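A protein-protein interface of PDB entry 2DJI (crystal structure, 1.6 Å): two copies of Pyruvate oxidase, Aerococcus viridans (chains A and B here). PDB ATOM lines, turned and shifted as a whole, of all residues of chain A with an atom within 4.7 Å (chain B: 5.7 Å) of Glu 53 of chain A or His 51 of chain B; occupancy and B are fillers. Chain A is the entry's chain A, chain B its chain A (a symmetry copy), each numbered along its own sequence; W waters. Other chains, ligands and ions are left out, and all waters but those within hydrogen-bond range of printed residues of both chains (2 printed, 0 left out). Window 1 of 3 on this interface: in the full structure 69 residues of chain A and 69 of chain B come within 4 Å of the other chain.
His 51 of chain A touches Glu 53 of chain B, and with the chains exchanged Glu 53 of chain A touches His 51 of chain B.
Glu 53 of chain A touches His 82 of chain B, and with the chains exchanged His 82 of chain A touches Glu 53 of chain B.
Of the 11 printed residues of chain A, 5 touch a printed residue of chain B.
Hydrophobic or aromatic side chains of chain A within 4 Å of the printed part of chain B: His 51, His 82 and Met 445.
Of the 11 printed residues of chain B, 6 touch a printed residue of chain A.
Hydrophobic or aromatic side chains of chain B within 4 Å of the printed part of chain A: Ile 25, His 51 and His 82.
Among the printed residues, 10 pairs touch across the chains.
Among the printed residues, no Asp or Glu carboxylate lies within 4 Å of a Lys or Arg side-chain nitrogen of the other chain.
Among the printed residues, merely in contact across the chains: Met 445 of chain A with Lys 50 of chain B (3.2 Å), Met 445 of chain A with Glu 52 of chain B (3.4 Å), Met 445 of chain A with Ile 25 of chain B (3.5 Å), Met 445 of chain A with His 51 of chain B (3.8 Å) and Met 445 of chain A with His 82 of chain B (3.9 Å).
Water W1 bridges the side-chain carboxylate (OE2) of Glu 53 of chain A and a ring nitrogen (NE2) of His 82 of chain B.
Water W2 lies within hydrogen-bond range of the side-chain carboxylate (OE2) of Glu 53 of chain B (3.1 Å) and a ring nitrogen (NE2) of His 82 of chain A (3.3 Å).
Glu 53 of chain A touches just these residues of chain B: His 51 (2.9 Å) and His 82 (2.7 Å).
His 51 of chain B touches just these residues of chain A: Glu 53 (2.9 Å) and Met 445 (3.8 Å).
Of the printed residues of chain B, His 82 of chain A touches Glu 53 (2.7 Å).
Of the printed residues of chain B, His 51 of chain A touches Glu 53 (2.9 Å).
Of the printed residues of chain B, Asn 85 of chain A touches His 82.
Printed residues of chain A within 4 Å of Glu 52 of chain B: Met 445.
The nearest residue of chain A that does not touch His 51 of chain B is His 51 of chain A (4.5 Å).
NE2 of His 51 of chain A lies within hydrogen-bond range of OE2 of Glu 53 of chain B (2.9 Å).
OE2 of Glu 53 of chain A is in hydrogen-bond range of NE2 of His 51 of chain B (2.9 Å).
A ring nitrogen (NE2) of His 82 of chain B lies within hydrogen-bond range of the side-chain carboxylate of Glu 53 of chain A (2.7 Å).
A ring nitrogen (NE2) of His 82 of chain A is in hydrogen-bond range of the side-chain carboxylate of Glu 53 of chain B.
The side-chain amide nitrogen (ND2) of Asn 85 of chain A lies within hydrogen-bond range of a ring nitrogen (NE2) of His 82 of chain B (3.3 Å).
ND1 of His 51 of chain A sits close to N of Glu 53 of chain A.
ND1 of His 82 of chain A lies within hydrogen-bond range of OE1 of Glu 52 of chain A (2.8 Å).
The backbone carbonyl oxygen (O) of His 82 of chain A sits close to the backbone NH (N) of Glu 53 of chain A, at 3.4 Å.
A ring nitrogen (ND1) of His 51 of chain B sits close to the backbone NH of Glu 53 of chain B (3.1 Å).
A ring nitrogen (NE2) of His 82 of chain B sits at hydrogen-bond distance from a ring nitrogen (NE2) of His 51 of chain B, 3.3 Å away.
N of His 51 of chain B sits at hydrogen-bond distance from OD2 of Asp 449 of chain B (3.3 Å).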
ATOM      1  N   HIS A  51      14.784  17.108  19.210  1.00  0.00           N
ATOM      2  CA  HIS A  51      13.347  16.859  19.336  1.00  0.00           C
ATOM      3  C   HIS A  51      13.074  15.538  18.622  1.00  0.00           C
ATOM      4  O   HIS A  51      13.468  15.360  17.467  1.00  0.00           O
ATOM      5  CB  HIS A  51      12.555  18.004  18.685  1.00  0.00           C
ATOM      6  CG  HIS A  51      11.092  18.002  19.016  1.00  0.00           C
ATOM      7  ND1 HIS A  51      10.234  17.001  18.610  1.00  0.00           N
ATOM      8  CD2 HIS A  51      10.332  18.897  19.691  1.00  0.00           C
ATOM      9  CE1 HIS A  51       9.010  17.280  19.021  1.00  0.00           C
ATOM     10  NE2 HIS A  51       9.042  18.426  19.680  1.00  0.00           N
ATOM     11  N   GLU A  52      12.412  14.610  19.308  1.00  0.00           N
ATOM     12  CA  GLU A  52      12.149  13.298  18.722  1.00  0.00           C
ATOM     13  C   GLU A  52      11.457  13.312  17.374  1.00  0.00           C
ATOM     14  O   GLU A  52      11.625  12.380  16.598  1.00  0.00           O
ATOM     15  CB  GLU A  52      11.341  12.410  19.676  1.00  0.00           C
ATOM     16  CG  GLU A  52      12.049  12.096  20.979  1.00  0.00           C
ATOM     17  CD  GLU A  52      11.695  13.079  22.072  1.00  0.00           C
ATOM     18  OE1 GLU A  52      11.240  14.193  21.744  1.00  0.00           O
ATOM     19  OE2 GLU A  52      11.880  12.739  23.258  1.00  0.00           O
ATOM     20  N   GLU A  53      10.678  14.348  17.081  1.00  0.00           N
ATOM     21  CA  GLU A  53      10.001  14.368  15.793  1.00  0.00           C
ATOM     22  C   GLU A  53      11.019  14.498  14.665  1.00  0.00           C
ATOM     23  O   GLU A  53      10.821  13.959  13.578  1.00  0.00           O
ATOM     24  CB  GLU A  53       8.960  15.495  15.730  1.00  0.00           C
ATOM     25  CG  GLU A  53       9.467  16.854  15.305  1.00  0.00           C
ATOM     26  CD  GLU A  53       8.324  17.832  15.106  1.00  0.00           C
ATOM     27  OE1 GLU A  53       7.318  17.446  14.471  1.00  0.00           O
ATOM     28  OE2 GLU A  53       8.426  18.981  15.572  1.00  0.00           O
ATOM     29  N   VAL A  54      12.117  15.202  14.929  1.00  0.00           N
ATOM     30  CA  VAL A  54      13.164  15.359  13.927  1.00  0.00           C
ATOM     31  C   VAL A  54      13.847  14.006  13.717  1.00  0.00           C
ATOM     32  O   VAL A  54      14.273  13.680  12.609  1.00  0.00           O
ATOM     33  CB  VAL A  54      14.197  16.427  14.365  1.00  0.00           C
ATOM     34  CG1 VAL A  54      15.398  16.435  13.411  1.00  0.00           C
ATOM     35  CG2 VAL A  54      13.527  17.801  14.368  1.00  0.00           C
ATOM     36  N   GLY A  55      13.937  13.218  14.788  1.00  0.00           N
ATOM     37  CA  GLY A  55      14.544  11.902  14.688  1.00  0.00           C
ATOM     38  C   GLY A  55      13.689  10.991  13.823  1.00  0.00           C
ATOM     39  O   GLY A  55      14.205  10.259  12.978  1.00  0.00           O
ATOM     40  N   ALA A  56      12.375  11.035  14.031  1.00  0.00           N
ATOM     41  CA  ALA A  56      11.460  10.212  13.248  1.00  0.00           C
ATOM     42  C   ALA A  56      11.489  10.641  11.783  1.00  0.00           C
ATOM     43  O   ALA A  56      11.602   9.806  10.885  1.00  0.00           O
ATOM     44  CB  ALA A  56      10.036  10.325  13.809  1.00  0.00           C
ATOM     45  N   MET A  57      11.405  11.946  11.541  1.00  0.00           N
ATOM     46  CA  MET A  57      11.426  12.447  10.173  1.00  0.00           C
ATOM     47  C   MET A  57      12.742  12.138   9.464  1.00  0.00           C
ATOM     48  O   MET A  57      12.753  11.853   8.268  1.00  0.00           O
ATOM     49  CB  MET A  57      11.170  13.957  10.150  1.00  0.00           C
ATOM     50  CG  MET A  57       9.720  14.327  10.421  1.00  0.00           C
ATOM     51  SD  MET A  57       9.415  16.108  10.298  1.00  0.00           S
ATOM     52  CE  MET A  57       9.953  16.642  11.856  1.00  0.00           C
ATOM     53  N   HIS A  82       5.969  12.166  20.367  1.00  0.00           N
ATOM     54  CA  HIS A  82       6.668  13.177  19.576  1.00  0.00           C
ATOM     55  C   HIS A  82       7.040  12.673  18.175  1.00  0.00           C
ATOM     56  O   HIS A  82       7.356  13.464  17.288  1.00  0.00           O
ATOM     57  CB  HIS A  82       7.935  13.634  20.306  1.00  0.00           C
ATOM     58  CG  HIS A  82       7.774  14.924  21.051  1.00  0.00           C
ATOM     59  ND1 HIS A  82       8.749  15.429  21.886  1.00  0.00           N
ATOM     60  CD2 HIS A  82       6.761  15.823  21.068  1.00  0.00           C
ATOM     61  CE1 HIS A  82       8.344  16.583  22.386  1.00  0.00           C
ATOM     62  NE2 HIS A  82       7.141  16.845  21.905  1.00  0.00           N
ATOM     63  N   LEU A  83       6.995  11.360  17.973  1.00  0.00           N
ATOM     64  CA  LEU A  83       7.337  10.784  16.673  1.00  0.00           C
ATOM     65  C   LEU A  83       6.217  10.914  15.646  1.00  0.00           C
ATOM     66  O   LEU A  83       6.448  10.750  14.452  1.00  0.00           O
ATOM     67  CB  LEU A  83       7.654   9.291  16.820  1.00  0.00           C
ATOM     68  CG  LEU A  83       8.638   8.825  17.893  1.00  0.00           C
ATOM     69  CD1 LEU A  83       8.712   7.304  17.862  1.00  0.00           C
ATOM     70  CD2 LEU A  83      10.005   9.442  17.655  1.00  0.00           C
ATOM     71  N   ASN A  85       4.377  13.154  13.751  1.00  0.00           N
ATOM     72  CA  ASN A  85       4.424  13.774  12.427  1.00  0.00           C
ATOM     73  C   ASN A  85       5.333  13.044  11.452  1.00  0.00           C
ATOM     74  O   ASN A  85       5.063  13.010  10.250  1.00  0.00           O
ATOM     75  CB  ASN A  85       4.827  15.242  12.536  1.00  0.00           C
ATOM     76  CG  ASN A  85       3.684  16.108  13.007  1.00  0.00           C
ATOM     77  OD1 ASN A  85       3.023  15.792  13.997  1.00  0.00           O
ATOM     78  ND2 ASN A  85       3.435  17.204  12.300  1.00  0.00           N
ATOM     79  N   MET A 445       9.867  25.747  13.633  1.00  0.00           N
ATOM     80  CA  MET A 445       9.414  24.529  14.297  1.00  0.00           C
ATOM     81  C   MET A 445      10.558  23.547  14.486  1.00  0.00           C
ATOM     82  O   MET A 445      10.439  22.592  15.254  1.00  0.00           O
ATOM     83  CB  MET A 445       8.323  23.847  13.476  1.00  0.00           C
ATOM     84  CG  MET A 445       7.050  24.639  13.353  1.00  0.00           C
ATOM     85  SD  MET A 445       5.769  23.651  12.566  1.00  0.00           S
ATOM     86  CE  MET A 445       4.375  24.800  12.631  1.00  0.00           C
ATOM     87  N   ILE B  25      -1.832  28.158  15.299  1.00  0.00           N
ATOM     88  CA  ILE B  25      -1.185  28.765  14.150  1.00  0.00           C
ATOM     89  C   ILE B  25      -2.208  28.868  13.024  1.00  0.00           C
ATOM     90  O   ILE B  25      -2.944  27.918  12.758  1.00  0.00           O
ATOM     91  CB  ILE B  25       0.004  27.899  13.679  1.00  0.00           C
ATOM     92  CG1 ILE B  25       1.012  27.754  14.822  1.00  0.00           C
ATOM     93  CG2 ILE B  25       0.658  28.523  12.458  1.00  0.00           C
ATOM     94  CD1 ILE B  25       2.209  26.892  14.487  1.00  0.00           C
ATOM     95  N   VAL B  49       1.391  30.752  18.212  1.00  0.00           N
ATOM     96  CA  VAL B  49       2.625  30.143  18.684  1.00  0.00           C
ATOM     97  C   VAL B  49       3.487  29.737  17.485  1.00  0.00           C
ATOM     98  O   VAL B  49       3.067  29.888  16.335  1.00  0.00           O
ATOM     99  CB  VAL B  49       2.324  28.899  19.546  1.00  0.00           C
ATOM    100  CG1 VAL B  49       1.606  29.314  20.822  1.00  0.00           C
ATOM    101  CG2 VAL B  49       1.464  27.913  18.753  1.00  0.00           C
ATOM    102  N   LYS B  50       4.691  29.235  17.748  1.00  0.00           N
ATOM    103  CA  LYS B  50       5.583  28.818  16.665  1.00  0.00           C
ATOM    104  C   LYS B  50       5.440  27.329  16.352  1.00  0.00           C
ATOM    105  O   LYS B  50       5.701  26.897  15.229  1.00  0.00           O
ATOM    106  CB  LYS B  50       7.040  29.127  17.016  1.00  0.00           C
ATOM    107  CG  LYS B  50       7.315  30.588  17.365  1.00  0.00           C
ATOM    108  CD  LYS B  50       6.693  31.551  16.356  1.00  0.00           C
ATOM    109  CE  LYS B  50       7.195  31.312  14.945  1.00  0.00           C
ATOM    110  NZ  LYS B  50       6.599  32.288  13.991  1.00  0.00           N
ATOM    111  N   HIS B  51       5.027  26.553  17.349  1.00  0.00           N
ATOM    112  CA  HIS B  51       4.834  25.110  17.184  1.00  0.00           C
ATOM    113  C   HIS B  51       3.509  24.772  17.860  1.00  0.00           C
ATOM    114  O   HIS B  51       3.289  25.132  19.019  1.00  0.00           O
ATOM    115  CB  HIS B  51       5.993  24.345  17.844  1.00  0.00           C
ATOM    116  CG  HIS B  51       6.053  22.892  17.480  1.00  0.00           C
ATOM    117  ND1 HIS B  51       5.076  21.989  17.841  1.00  0.00           N
ATOM    118  CD2 HIS B  51       6.992  22.182  16.809  1.00  0.00           C
ATOM    119  CE1 HIS B  51       5.411  20.786  17.409  1.00  0.00           C
ATOM    120  NE2 HIS B  51       6.569  20.876  16.779  1.00  0.00           N
ATOM    121  N   GLU B  52       2.622  24.093  17.137  1.00  0.00           N
ATOM    122  CA  GLU B  52       1.308  23.767  17.685  1.00  0.00           C
ATOM    123  C   GLU B  52       1.316  23.044  19.016  1.00  0.00           C
ATOM    124  O   GLU B  52       0.361  23.160  19.773  1.00  0.00           O
ATOM    125  CB  GLU B  52       0.473  22.950  16.691  1.00  0.00           C
ATOM    126  CG  GLU B  52       0.163  23.678  15.399  1.00  0.00           C
ATOM    127  CD  GLU B  52       1.183  23.386  14.321  1.00  0.00           C
ATOM    128  OE1 GLU B  52       2.305  22.965  14.665  1.00  0.00           O
ATOM    129  OE2 GLU B  52       0.864  23.586  13.132  1.00  0.00           O
ATOM    130  N   GLU B  53       2.374  22.297  19.316  1.00  0.00           N
ATOM    131  CA  GLU B  53       2.390  21.591  20.589  1.00  0.00           C
ATOM    132  C   GLU B  53       2.455  22.586  21.742  1.00  0.00           C
ATOM    133  O   GLU B  53       1.899  22.342  22.812  1.00  0.00           O
ATOM    134  CB  GLU B  53       3.553  20.591  20.655  1.00  0.00           C
ATOM    135  CG  GLU B  53       4.882  21.138  21.123  1.00  0.00           C
ATOM    136  CD  GLU B  53       5.897  20.027  21.319  1.00  0.00           C
ATOM    137  OE1 GLU B  53       5.534  18.992  21.922  1.00  0.00           O
ATOM    138  OE2 GLU B  53       7.052  20.183  20.883  1.00  0.00           O
ATOM    139  N   VAL B  54       3.124  23.715  21.521  1.00  0.00           N
ATOM    140  CA  VAL B  54       3.218  24.742  22.550  1.00  0.00           C
ATOM    141  C   VAL B  54       1.836  25.371  22.743  1.00  0.00           C
ATOM    142  O   VAL B  54       1.469  25.757  23.853  1.00  0.00           O
ATOM    143  CB  VAL B  54       4.256  25.824  22.162  1.00  0.00           C
ATOM    144  CG1 VAL B  54       4.197  27.002  23.143  1.00  0.00           C
ATOM    145  CG2 VAL B  54       5.655  25.206  22.176  1.00  0.00           C
ATOM    146  N   GLY B  55       1.071  25.457  21.656  1.00  0.00           N
ATOM    147  CA  GLY B  55      -0.270  26.012  21.739  1.00  0.00           C
ATOM    148  C   GLY B  55      -1.168  25.104  22.561  1.00  0.00           C
ATOM    149  O   GLY B  55      -1.938  25.573  23.400  1.00  0.00           O
ATOM    150  N   ALA B  56      -1.070  23.797  22.325  1.00  0.00           N
ATOM    151  CA  ALA B  56      -1.875  22.834  23.067  1.00  0.00           C
ATOM    152  C   ALA B  56      -1.482  22.845  24.542  1.00  0.00           C
ATOM    153  O   ALA B  56      -2.341  22.905  25.422  1.00  0.00           O
ATOM    154  CB  ALA B  56      -1.696  21.429  22.476  1.00  0.00           C
ATOM    155  N   HIS B  82       0.446  17.591  15.871  1.00  0.00           N
ATOM    156  CA  HIS B  82       1.412  18.308  16.703  1.00  0.00           C
ATOM    157  C   HIS B  82       0.861  18.627  18.099  1.00  0.00           C
ATOM    158  O   HIS B  82       1.619  18.951  19.012  1.00  0.00           O
ATOM    159  CB  HIS B  82       1.837  19.608  16.013  1.00  0.00           C
ATOM    160  CG  HIS B  82       3.149  19.512  15.295  1.00  0.00           C
ATOM    161  ND1 HIS B  82       3.636  20.525  14.495  1.00  0.00           N
ATOM    162  CD2 HIS B  82       4.086  18.534  15.276  1.00  0.00           C
ATOM    163  CE1 HIS B  82       4.816  20.175  14.014  1.00  0.00           C
ATOM    164  NE2 HIS B  82       5.112  18.971  14.473  1.00  0.00           N
ATOM    165  N   ASP B 449       9.761  29.225  20.773  1.00  0.00           N
ATOM    166  CA  ASP B 449       8.572  29.932  21.232  1.00  0.00           C
ATOM    167  C   ASP B 449       8.831  31.025  22.265  1.00  0.00           C
ATOM    168  O   ASP B 449       7.901  31.637  22.790  1.00  0.00           O
ATOM    169  CB  ASP B 449       7.519  28.939  21.733  1.00  0.00           C
ATOM    170  CG  ASP B 449       6.501  28.603  20.660  1.00  0.00           C
ATOM    171  OD1 ASP B 449       5.663  29.479  20.349  1.00  0.00           O
ATOM    172  OD2 ASP B 449       6.546  27.481  20.113  1.00  0.00           O
HETATM  173  O   HOH W   1       7.704  20.354  12.924  1.00  0.00           O
HETATM  174  O   HOH W   2       8.389  19.448  23.547  1.00  0.00           O
